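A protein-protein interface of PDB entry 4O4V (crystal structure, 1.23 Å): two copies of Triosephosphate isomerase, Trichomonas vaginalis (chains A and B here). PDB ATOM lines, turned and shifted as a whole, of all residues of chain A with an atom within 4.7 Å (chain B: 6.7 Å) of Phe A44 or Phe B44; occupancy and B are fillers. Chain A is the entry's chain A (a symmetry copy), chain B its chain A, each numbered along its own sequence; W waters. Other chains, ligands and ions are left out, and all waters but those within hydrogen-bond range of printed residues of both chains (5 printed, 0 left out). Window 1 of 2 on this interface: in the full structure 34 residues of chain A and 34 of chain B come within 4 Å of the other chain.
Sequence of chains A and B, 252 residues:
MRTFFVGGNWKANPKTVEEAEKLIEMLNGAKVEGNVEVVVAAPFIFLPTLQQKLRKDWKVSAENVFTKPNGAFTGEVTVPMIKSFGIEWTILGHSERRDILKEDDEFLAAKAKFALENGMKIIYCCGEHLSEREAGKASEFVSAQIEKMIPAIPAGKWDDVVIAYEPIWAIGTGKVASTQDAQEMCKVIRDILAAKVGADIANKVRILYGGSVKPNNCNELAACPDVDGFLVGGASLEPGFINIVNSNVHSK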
ATOM      1  N   ALA A  42      -9.343 -16.632 -21.646  1.00  0.00           N
ATOM      2  CA  ALA A  42      -9.440 -15.697 -22.768  1.00  0.00           C
ATOM      3  C   ALA A  42      -8.146 -14.916 -22.911  1.00  0.00           C
ATOM      4  O   ALA A  42      -7.345 -14.848 -21.971  1.00  0.00           O
ATOM      5  CB  ALA A  42     -10.600 -14.763 -22.545  1.00  0.00           C
ATOM      6  N   PRO A  43      -7.959 -14.246 -24.052  1.00  0.00           N
ATOM      7  CA  PRO A  43      -6.785 -13.371 -24.226  1.00  0.00           C
ATOM      8  C   PRO A  43      -6.707 -12.296 -23.159  1.00  0.00           C
ATOM      9  O   PRO A  43      -7.729 -11.779 -22.692  1.00  0.00           O
ATOM     10  CB  PRO A  43      -7.017 -12.752 -25.611  1.00  0.00           C
ATOM     11  CG  PRO A  43      -7.812 -13.789 -26.338  1.00  0.00           C
ATOM     12  CD  PRO A  43      -8.717 -14.387 -25.312  1.00  0.00           C
ATOM     13  N   PHE A  44      -5.489 -11.902 -22.806  1.00  0.00           N
ATOM     14  CA  PHE A  44      -5.289 -10.954 -21.719  1.00  0.00           C
ATOM     15  C   PHE A  44      -6.146  -9.714 -21.843  1.00  0.00           C
ATOM     16  O   PHE A  44      -6.701  -9.231 -20.853  1.00  0.00           O
ATOM     17  CB  PHE A  44      -3.833 -10.484 -21.635  1.00  0.00           C
ATOM     18  CG  PHE A  44      -2.823 -11.528 -21.265  1.00  0.00           C
ATOM     19  CD1 PHE A  44      -2.885 -12.203 -20.057  1.00  0.00           C
ATOM     20  CD2 PHE A  44      -1.770 -11.793 -22.108  1.00  0.00           C
ATOM     21  CE1 PHE A  44      -1.890 -13.140 -19.719  1.00  0.00           C
ATOM     22  CE2 PHE A  44      -0.779 -12.723 -21.768  1.00  0.00           C
ATOM     23  CZ  PHE A  44      -0.858 -13.384 -20.582  1.00  0.00           C
ATOM     24  N   ILE A  45      -6.218  -9.160 -23.057  1.00  0.00           N
ATOM     25  CA  ILE A  45      -6.877  -7.883 -23.270  1.00  0.00           C
ATOM     26  C   ILE A  45      -8.396  -7.983 -23.102  1.00  0.00           C
ATOM     27  O   ILE A  45      -9.063  -6.951 -22.902  1.00  0.00           O
ATOM     28  CB  ILE A  45      -6.468  -7.323 -24.646  1.00  0.00           C
ATOM     29  CG1 ILE A  45      -6.765  -5.822 -24.735  1.00  0.00           C
ATOM     30  CG2 ILE A  45      -7.094  -8.098 -25.793  1.00  0.00           C
ATOM     31  CD1 ILE A  45      -6.263  -5.165 -26.033  1.00  0.00           C
ATOM     32  N   PHE A  46      -8.940  -9.190 -23.159  1.00  0.00           N
ATOM     33  CA  PHE A  46     -10.360  -9.421 -22.906  1.00  0.00           C
ATOM     34  C   PHE A  46     -10.657  -9.857 -21.472  1.00  0.00           C
ATOM     35  O   PHE A  46     -11.827  -9.957 -21.089  1.00  0.00           O
ATOM     36  CB  PHE A  46     -10.929 -10.489 -23.852  1.00  0.00           C
ATOM     37  CG  PHE A  46     -10.880 -10.138 -25.319  1.00  0.00           C
ATOM     38  CD1 PHE A  46     -10.991  -8.834 -25.784  1.00  0.00           C
ATOM     39  CD2 PHE A  46     -10.727 -11.142 -26.259  1.00  0.00           C
ATOM     40  CE1 PHE A  46     -10.928  -8.558 -27.171  1.00  0.00           C
ATOM     41  CE2 PHE A  46     -10.667 -10.862 -27.635  1.00  0.00           C
ATOM     42  CZ  PHE A  46     -10.791  -9.574 -28.080  1.00  0.00           C
ATOM     43  N   LEU A  47      -9.646 -10.102 -20.655  1.00  0.00           N
ATOM     44  CA  LEU A  47      -9.900 -10.575 -19.301  1.00  0.00           C
ATOM     45  C   LEU A  47     -10.722  -9.595 -18.463  1.00  0.00           C
ATOM     46  O   LEU A  47     -11.593 -10.035 -17.726  1.00  0.00           O
ATOM     47  CB  LEU A  47      -8.602 -10.944 -18.585  1.00  0.00           C
ATOM     48  CG  LEU A  47      -7.870 -12.195 -19.125  1.00  0.00           C
ATOM     49  CD1 LEU A  47      -6.568 -12.387 -18.400  1.00  0.00           C
ATOM     50  CD2 LEU A  47      -8.690 -13.451 -19.009  1.00  0.00           C
ATOM     51  N   PRO A  48     -10.465  -8.274 -18.550  1.00  0.00           N
ATOM     52  CA  PRO A  48     -11.318  -7.378 -17.759  1.00  0.00           C
ATOM     53  C   PRO A  48     -12.803  -7.484 -18.095  1.00  0.00           C
ATOM     54  O   PRO A  48     -13.640  -7.501 -17.208  1.00  0.00           O
ATOM     55  CB  PRO A  48     -10.723  -5.996 -18.020  1.00  0.00           C
ATOM     56  CG  PRO A  48      -9.277  -6.284 -18.331  1.00  0.00           C
ATOM     57  CD  PRO A  48      -9.342  -7.544 -19.168  1.00  0.00           C
ATOM     58  N   ALA A  62      -6.604 -16.712 -17.050  1.00  0.00           N
ATOM     59  CA  ALA A  62      -5.621 -16.343 -18.056  1.00  0.00           C
ATOM     60  C   ALA A  62      -5.149 -17.541 -18.846  1.00  0.00           C
ATOM     61  O   ALA A  62      -5.360 -18.701 -18.455  1.00  0.00           O
ATOM     62  CB  ALA A  62      -4.428 -15.665 -17.392  1.00  0.00           C
ATOM     63  N   ASN A  64      -1.836 -17.755 -19.849  1.00  0.00           N
ATOM     64  CA  ASN A  64      -0.401 -17.785 -19.572  1.00  0.00           C
ATOM     65  C   ASN A  64      -0.129 -16.734 -18.498  1.00  0.00           C
ATOM     66  O   ASN A  64      -0.933 -15.813 -18.333  1.00  0.00           O
ATOM     67  CB  ASN A  64       0.403 -17.448 -20.836  1.00  0.00           C
ATOM     68  CG  ASN A  64       1.888 -17.554 -20.642  1.00  0.00           C
ATOM     69  OD1 ASN A  64       2.362 -18.463 -19.993  1.00  0.00           O
ATOM     70  ND2 ASN A  64       2.625 -16.598 -21.215  1.00  0.00           N
ATOM     71  N   GLY A  75       6.077  -6.646 -22.742  1.00  0.00           N
ATOM     72  CA  GLY A  75       5.128  -7.549 -23.377  1.00  0.00           C
ATOM     73  C   GLY A  75       4.513  -8.590 -22.466  1.00  0.00           C
ATOM     74  O   GLY A  75       3.503  -9.188 -22.854  1.00  0.00           O
ATOM     75  N   VAL A  77       2.589 -10.224 -19.086  1.00  0.00           N
ATOM     76  CA  VAL A  77       1.573  -9.979 -18.058  1.00  0.00           C
ATOM     77  C   VAL A  77       1.859 -10.882 -16.881  1.00  0.00           C
ATOM     78  O   VAL A  77       2.262 -12.031 -17.049  1.00  0.00           O
ATOM     79  CB  VAL A  77       0.153 -10.220 -18.625  1.00  0.00           C
ATOM     80  CG1 VAL A  77      -0.911 -10.140 -17.543  1.00  0.00           C
ATOM     81  CG2 VAL A  77      -0.124  -9.195 -19.730  1.00  0.00           C
ATOM     82  N   ILE A  82      -3.163  -9.839 -13.010  1.00  0.00           N
ATOM     83  CA  ILE A  82      -4.345 -10.665 -13.200  1.00  0.00           C
ATOM     84  C   ILE A  82      -5.151 -10.731 -11.909  1.00  0.00           C
ATOM     85  O   ILE A  82      -6.373 -10.549 -11.917  1.00  0.00           O
ATOM     86  CB  ILE A  82      -3.909 -12.051 -13.700  1.00  0.00           C
ATOM     87  CG1 ILE A  82      -3.292 -11.947 -15.109  1.00  0.00           C
ATOM     88  CG2 ILE A  82      -5.058 -13.046 -13.678  1.00  0.00           C
ATOM     89  CD1 ILE A  82      -2.376 -13.115 -15.419  1.00  0.00           C
ATOM     90  N   ALA B  42       1.486  -0.096 -22.239  1.00  0.00           N
ATOM     91  CA  ALA B  42       1.169  -0.756 -20.971  1.00  0.00           C
ATOM     92  C   ALA B  42       0.924  -2.236 -21.198  1.00  0.00           C
ATOM     93  O   ALA B  42       0.662  -2.665 -22.328  1.00  0.00           O
ATOM     94  CB  ALA B  42      -0.042  -0.107 -20.355  1.00  0.00           C
ATOM     95  N   PRO B  43       0.919  -3.028 -20.121  1.00  0.00           N
ATOM     96  CA  PRO B  43       0.575  -4.457 -20.241  1.00  0.00           C
ATOM     97  C   PRO B  43      -0.799  -4.667 -20.850  1.00  0.00           C
ATOM     98  O   PRO B  43      -1.728  -3.882 -20.628  1.00  0.00           O
ATOM     99  CB  PRO B  43       0.608  -4.944 -18.786  1.00  0.00           C
ATOM    100  CG  PRO B  43       1.600  -4.038 -18.128  1.00  0.00           C
ATOM    101  CD  PRO B  43       1.398  -2.701 -18.763  1.00  0.00           C
ATOM    102  N   PHE B  44      -0.959  -5.767 -21.577  1.00  0.00           N
ATOM    103  CA  PHE B  44      -2.200  -6.021 -22.296  1.00  0.00           C
ATOM    104  C   PHE B  44      -3.432  -5.866 -21.434  1.00  0.00           C
ATOM    105  O   PHE B  44      -4.440  -5.305 -21.871  1.00  0.00           O
ATOM    106  CB  PHE B  44      -2.239  -7.437 -22.880  1.00  0.00           C
ATOM    107  CG  PHE B  44      -1.242  -7.732 -23.960  1.00  0.00           C
ATOM    108  CD1 PHE B  44      -1.229  -7.025 -25.151  1.00  0.00           C
ATOM    109  CD2 PHE B  44      -0.349  -8.766 -23.805  1.00  0.00           C
ATOM    110  CE1 PHE B  44      -0.311  -7.364 -26.164  1.00  0.00           C
ATOM    111  CE2 PHE B  44       0.560  -9.104 -24.816  1.00  0.00           C
ATOM    112  CZ  PHE B  44       0.566  -8.395 -25.976  1.00  0.00           C
ATOM    113  N   ILE B  45      -3.376  -6.409 -20.213  1.00  0.00           N
ATOM    114  CA  ILE B  45      -4.547  -6.465 -19.354  1.00  0.00           C
ATOM    115  C   ILE B  45      -4.952  -5.080 -18.842  1.00  0.00           C
ATOM    116  O   ILE B  45      -6.102  -4.899 -18.399  1.00  0.00           O
ATOM    117  CB  ILE B  45      -4.291  -7.468 -18.213  1.00  0.00           C
ATOM    118  CG1 ILE B  45      -5.609  -7.892 -17.553  1.00  0.00           C
ATOM    119  CG2 ILE B  45      -3.287  -6.945 -17.199  1.00  0.00           C
ATOM    120  CD1 ILE B  45      -5.445  -8.992 -16.491  1.00  0.00           C
ATOM    121  N   PHE B  46      -4.049  -4.112 -18.912  1.00  0.00           N
ATOM    122  CA  PHE B  46      -4.355  -2.729 -18.555  1.00  0.00           C
ATOM    123  C   PHE B  46      -4.711  -1.858 -19.758  1.00  0.00           C
ATOM    124  O   PHE B  46      -5.119  -0.705 -19.583  1.00  0.00           O
ATOM    125  CB  PHE B  46      -3.176  -2.068 -17.824  1.00  0.00           C
ATOM    126  CG  PHE B  46      -2.802  -2.702 -16.507  1.00  0.00           C
ATOM    127  CD1 PHE B  46      -3.731  -3.311 -15.674  1.00  0.00           C
ATOM    128  CD2 PHE B  46      -1.483  -2.680 -16.087  1.00  0.00           C
ATOM    129  CE1 PHE B  46      -3.324  -3.901 -14.453  1.00  0.00           C
ATOM    130  CE2 PHE B  46      -1.086  -3.266 -14.873  1.00  0.00           C
ATOM    131  CZ  PHE B  46      -2.015  -3.851 -14.055  1.00  0.00           C
ATOM    132  N   LEU B  47      -4.594  -2.365 -20.973  1.00  0.00           N
ATOM    133  CA  LEU B  47      -4.871  -1.538 -22.140  1.00  0.00           C
ATOM    134  C   LEU B  47      -6.306  -1.011 -22.180  1.00  0.00           C
ATOM    135  O   LEU B  47      -6.501   0.141 -22.540  1.00  0.00           O
ATOM    136  CB  LEU B  47      -4.524  -2.267 -23.437  1.00  0.00           C
ATOM    137  CG  LEU B  47      -3.017  -2.510 -23.688  1.00  0.00           C
ATOM    138  CD1 LEU B  47      -2.824  -3.316 -24.942  1.00  0.00           C
ATOM    139  CD2 LEU B  47      -2.227  -1.236 -23.795  1.00  0.00           C
ATOM    140  N   PRO B  48      -7.320  -1.827 -21.826  1.00  0.00           N
ATOM    141  CA  PRO B  48      -8.670  -1.252 -21.838  1.00  0.00           C
ATOM    142  C   PRO B  48      -8.835  -0.045 -20.920  1.00  0.00           C
ATOM    143  O   PRO B  48      -9.448   0.941 -21.293  1.00  0.00           O
ATOM    144  CB  PRO B  48      -9.565  -2.434 -21.472  1.00  0.00           C
ATOM    145  CG  PRO B  48      -8.784  -3.632 -21.947  1.00  0.00           C
ATOM    146  CD  PRO B  48      -7.355  -3.284 -21.592  1.00  0.00           C
ATOM    147  N   ALA B  62       0.234  -1.010 -27.360  1.00  0.00           N
ATOM    148  CA  ALA B  62       0.643  -2.307 -26.846  1.00  0.00           C
ATOM    149  C   ALA B  62       2.145  -2.427 -26.753  1.00  0.00           C
ATOM    150  O   ALA B  62       2.898  -1.629 -27.337  1.00  0.00           O
ATOM    151  CB  ALA B  62       0.093  -3.415 -27.737  1.00  0.00           C
ATOM    152  N   GLU B  63       2.619  -3.433 -26.038  1.00  0.00           N
ATOM    153  CA  GLU B  63       4.044  -3.687 -25.844  1.00  0.00           C
ATOM    154  C   GLU B  63       4.585  -4.802 -26.743  1.00  0.00           C
ATOM    155  O   GLU B  63       5.792  -5.061 -26.769  1.00  0.00           O
ATOM    156  CB  GLU B  63       4.365  -4.021 -24.386  1.00  0.00           C
ATOM    157  CG  GLU B  63       4.188  -2.815 -23.438  1.00  0.00           C
ATOM    158  CD  GLU B  63       4.529  -3.135 -21.998  1.00  0.00           C
ATOM    159  OE1 GLU B  63       5.231  -4.119 -21.727  1.00  0.00           O
ATOM    160  OE2 GLU B  63       4.068  -2.354 -21.096  1.00  0.00           O
ATOM    161  N   ASN B  64       3.685  -5.453 -27.466  1.00  0.00           N
ATOM    162  CA  ASN B  64       3.978  -6.577 -28.353  1.00  0.00           C
ATOM    163  C   ASN B  64       2.676  -6.940 -29.063  1.00  0.00           C
ATOM    164  O   ASN B  64       1.598  -6.605 -28.563  1.00  0.00           O
ATOM    165  CB  ASN B  64       4.480  -7.785 -27.551  1.00  0.00           C
ATOM    166  CG  ASN B  64       4.889  -8.944 -28.414  1.00  0.00           C
ATOM    167  OD1 ASN B  64       5.499  -8.758 -29.447  1.00  0.00           O
ATOM    168  ND2 ASN B  64       4.535 -10.156 -27.977  1.00  0.00           N
ATOM    169  N   VAL B  65       2.773  -7.689 -30.155  1.00  0.00           N
ATOM    170  CA  VAL B  65       1.619  -8.331 -30.803  1.00  0.00           C
ATOM    171  C   VAL B  65       2.117  -9.610 -31.440  1.00  0.00           C
ATOM    172  O   VAL B  65       3.319  -9.785 -31.676  1.00  0.00           O
ATOM    173  CB  VAL B  65       0.964  -7.454 -31.898  1.00  0.00           C
ATOM    174  CG1 VAL B  65       0.463  -6.157 -31.369  1.00  0.00           C
ATOM    175  CG2 VAL B  65       1.893  -7.193 -33.058  1.00  0.00           C
ATOM    176  N   PHE B  66       1.211 -10.529 -31.748  1.00  0.00           N
ATOM    177  CA  PHE B  66       1.580 -11.738 -32.474  1.00  0.00           C
ATOM    178  C   PHE B  66       1.541 -11.497 -34.001  1.00  0.00           C
ATOM    179  O   PHE B  66       1.287 -10.402 -34.453  1.00  0.00           O
ATOM    180  CB  PHE B  66       0.667 -12.898 -32.009  1.00  0.00           C
ATOM    181  CG  PHE B  66       1.115 -14.251 -32.456  1.00  0.00           C
ATOM    182  CD1 PHE B  66       2.354 -14.762 -32.121  1.00  0.00           C
ATOM    183  CD2 PHE B  66       0.274 -15.046 -33.234  1.00  0.00           C
ATOM    184  CE1 PHE B  66       2.745 -16.005 -32.541  1.00  0.00           C
ATOM    185  CE2 PHE B  66       0.675 -16.279 -33.653  1.00  0.00           C
ATOM    186  CZ  PHE B  66       1.889 -16.761 -33.327  1.00  0.00           C
ATOM    187  N   GLY B  75      -2.294 -17.854 -25.256  1.00  0.00           N
ATOM    188  CA  GLY B  75      -1.500 -16.847 -24.567  1.00  0.00           C
ATOM    189  C   GLY B  75      -1.193 -15.600 -25.369  1.00  0.00           C
ATOM    190  O   GLY B  75      -0.786 -14.600 -24.768  1.00  0.00           O
ATOM    191  N   GLU B  76      -1.362 -15.635 -26.690  1.00  0.00           N
ATOM    192  CA  GLU B  76      -1.014 -14.493 -27.540  1.00  0.00           C
ATOM    193  C   GLU B  76      -2.183 -13.522 -27.709  1.00  0.00           C
ATOM    194  O   GLU B  76      -3.332 -13.916 -27.778  1.00  0.00           O
ATOM    195  CB  GLU B  76      -0.539 -14.974 -28.911  1.00  0.00           C
ATOM    196  CG  GLU B  76       0.756 -15.757 -28.874  1.00  0.00           C
ATOM    197  CD  GLU B  76       1.921 -14.948 -28.291  1.00  0.00           C
ATOM    198  OE1 GLU B  76       2.252 -13.861 -28.837  1.00  0.00           O
ATOM    199  OE2 GLU B  76       2.522 -15.391 -27.279  1.00  0.00           O
ATOM    200  N   VAL B  77      -1.851 -12.242 -27.837  1.00  0.00           N
ATOM    201  CA  VAL B  77      -2.799 -11.176 -28.170  1.00  0.00           C
ATOM    202  C   VAL B  77      -2.484 -10.675 -29.560  1.00  0.00           C
ATOM    203  O   VAL B  77      -1.321 -10.571 -29.945  1.00  0.00           O
ATOM    204  CB  VAL B  77      -2.728 -10.035 -27.126  1.00  0.00           C
ATOM    205  CG1 VAL B  77      -3.574  -8.840 -27.533  1.00  0.00           C
ATOM    206  CG2 VAL B  77      -3.177 -10.575 -25.765  1.00  0.00           C
ATOM    207  N   THR B  78      -3.522 -10.422 -30.349  1.00  0.00           N
ATOM    208  CA  THR B  78      -3.353 -10.121 -31.768  1.00  0.00           C
ATOM    209  C   THR B  78      -3.797  -8.702 -32.112  1.00  0.00           C
ATOM    210  O   THR B  78      -4.534  -8.021 -31.375  1.00  0.00           O
ATOM    211  CB  THR B  78      -4.118 -11.117 -32.607  1.00  0.00           C
ATOM    212  OG1 THR B  78      -5.521 -10.897 -32.394  1.00  0.00           O
ATOM    213  CG2 THR B  78      -3.738 -12.552 -32.276  1.00  0.00           C
ATOM    214  N   MET B  81      -7.510  -7.636 -31.962  1.00  0.00           N
ATOM    215  CA  MET B  81      -8.041  -7.508 -30.604  1.00  0.00           C
ATOM    216  C   MET B  81      -7.726  -6.116 -30.069  1.00  0.00           C
ATOM    217  O   MET B  81      -8.576  -5.447 -29.479  1.00  0.00           O
ATOM    218  CB  MET B  81      -7.433  -8.551 -29.687  1.00  0.00           C
ATOM    219  CG  MET B  81      -7.676  -9.996 -30.058  1.00  0.00           C
ATOM    220  SD  MET B  81      -6.731 -11.066 -28.954  1.00  0.00           S
ATOM    221  CE  MET B  81      -6.992 -12.661 -29.753  1.00  0.00           C
ATOM    222  N   ILE B  82      -6.486  -5.693 -30.241  1.00  0.00           N
ATOM    223  CA  ILE B  82      -6.021  -4.389 -29.797  1.00  0.00           C
ATOM    224  C   ILE B  82      -6.767  -3.287 -30.541  1.00  0.00           C
ATOM    225  O   ILE B  82      -7.252  -2.329 -29.930  1.00  0.00           O
ATOM    226  CB  ILE B  82      -4.499  -4.310 -29.990  1.00  0.00           C
ATOM    227  CG1 ILE B  82      -3.785  -5.303 -29.051  1.00  0.00           C
ATOM    228  CG2 ILE B  82      -3.977  -2.896 -29.791  1.00  0.00           C
ATOM    229  CD1 ILE B  82      -2.401  -5.669 -29.554  1.00  0.00           C
ATOM    230  N   THR B  90       1.854  -0.309 -31.441  1.00  0.00           N
ATOM    231  CA  THR B  90       2.557  -1.341 -30.681  1.00  0.00           C
ATOM    232  C   THR B  90       4.056  -1.122 -30.738  1.00  0.00           C
ATOM    233  O   THR B  90       4.600  -0.659 -31.751  1.00  0.00           O
ATOM    234  CB  THR B  90       2.228  -2.778 -31.162  1.00  0.00           C
ATOM    235  OG1 THR B  90       2.756  -3.738 -30.228  1.00  0.00           O
ATOM    236  CG2 THR B  90       2.702  -3.054 -32.556  1.00  0.00           C
ATOM    237  N   ARG B  97      12.325  -8.669 -25.195  1.00  0.00           N
ATOM    238  CA  ARG B  97      11.701  -9.734 -25.954  1.00  0.00           C
ATOM    239  C   ARG B  97      12.676 -10.488 -26.857  1.00  0.00           C
ATOM    240  O   ARG B  97      12.570 -11.709 -27.007  1.00  0.00           O
ATOM    241  CB  ARG B  97      10.492  -9.247 -26.729  1.00  0.00           C
ATOM    242  CG  ARG B  97       9.447  -8.625 -25.818  1.00  0.00           C
ATOM    243  CD  ARG B  97       8.039  -8.712 -26.370  1.00  0.00           C
ATOM    244  NE  ARG B  97       7.570 -10.089 -26.526  1.00  0.00           N
ATOM    245  CZ  ARG B  97       7.112 -10.849 -25.539  1.00  0.00           C
ATOM    246  NH1 ARG B  97       7.000 -10.370 -24.317  1.00  0.00           N
ATOM    247  NH2 ARG B  97       6.740 -12.098 -25.795  1.00  0.00           N
HETATM  248  O   HOH W   1       1.717  -6.758 -22.498  1.00  0.00           O
HETATM  249  O   HOH W   2      -3.500 -14.025 -23.533  1.00  0.00           O
HETATM  250  O   HOH W   3       1.634 -14.539 -23.100  1.00  0.00           O
HETATM  251  O   HOH W   4       3.363 -10.770 -25.327  1.00  0.00           O
HETATM  252  O   HOH W   5       3.501  -6.031 -20.529  1.00  0.00           O
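N of Gly A75 sits at hydrogen-bond distance from OE1 of Glu B63, 2.9 Å away.
The side-chain amide nitrogen (ND2) of Asn B64 sits close to the guanidinium group (NE) of Arg B97, 3.4 Å away. The backbone NH (N) of Phe B66 lies within hydrogen-bond range of the backbone carbonyl oxygen (O) of Val B77, at 3.1 Å. SD of Met B81 sits at hydrogen-bond distance from N of Thr B78 (3.6 Å).
Among the printed residues, pairs that only touch across the chains: Pro A43 with Met B81 (3.7 Å), Phe A44 with Phe B44 (3.7 Å), Phe A44 with Ile B45 (3.7 Å), Phe A44 with Gly B75 (3.5 Å), Phe A44 with Val B77 (3.98 Å), Ile A45 with Phe B44 (3.7 Å), Ile A45 with Pro B48 (3.5 Å), Ile A45 with Val B77 (3.996 Å), Ile A45 with Met B81 (3.9 Å), Ile A45 with Ile B82 (3.9 Å), Phe A46 with Met B81 (3.7 Å), Pro A48 with Ile B45 (3.5 Å), Gly A75 with Phe B44 (3.5 Å), Gly A75 with Arg B97 (3.5 Å), Val A77 with Phe B44 (3.98 Å), Val A77 with Ile B45 (3.996 Å) and Ile A82 with Ile B45 (3.9 Å).
Printed residues of chain B within 4 Å of Phe A44: Phe B44, Ile B45, Gly B75 and Val B77. Of the printed residues of chain A, Phe B44 touches Phe A44, Ile A45, Gly A75 and Val A77. Printed residues of chain A within 4 Å of Pro B48: Ile A45 (3.5 Å). Of the printed residues of chain B, Pro A43 touches Met B81 (3.7 Å). The nearest printed residue of chain A that does not touch Gly B75 is Asn A64 (4.2 Å).
Of the 20 printed residues of chain B, 9 touch a printed residue of chain A. Hydrophobic or aromatic side chains of chain B that line the printed part of chain A: Phe B44, Ile B45, Pro B48, Val B77, Met B81 and Ile B82. Of the 12 printed residues of chain A, 8 touch a printed residue of chain B. Hydrophobic or aromatic side chains of chain A that line the printed part of chain B: Pro A43, Phe A44, Ile A45, Phe A46, Pro A48, Val A77 and Ile A82. Among the printed residues, 18 pairs touch across the chains. Among the printed residues, no Asp or Glu carboxylate lies within 4 Å of a Lys or Arg side-chain nitrogen of the other chain.
Phe A44 touches Ile B45, and with the chains exchanged Ile A45 touches Phe B44. Phe A44 touches Gly B75, and with the chains exchanged Gly A75 touches Phe B44. Phe A44 touches Val B77, and with the chains exchanged Val A77 touches Phe B44. Ile A45 touches Ile B82, and with the chains exchanged Ile A82 touches Ile B45. 12 positions are printed for both chains. Of the 18 pairs that touch across the chains among the printed residues, 13 have their exchanged pair printed and touching as well.
Water W5 lies within hydrogen-bond range of the side-chain carboxylate of Glu B63 (2.8 Å) and the backbone NH of Gly A75 (3.5 Å). Water W3 lies within hydrogen-bond range of O of Gly B75 (2.9 Å) and ND2 of Asn A64 (3.0 Å). Water W4 lies within hydrogen-bond range of O of Gly A75 (2.9 Å) and ND2 of Asn B64 (3.0 Å). Water W2 bridges N of Phe A44 (3.0 Å) and O of Gly B75 (3.0 Å). Water W1 bridges N of Phe B44 and O of Gly A75.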
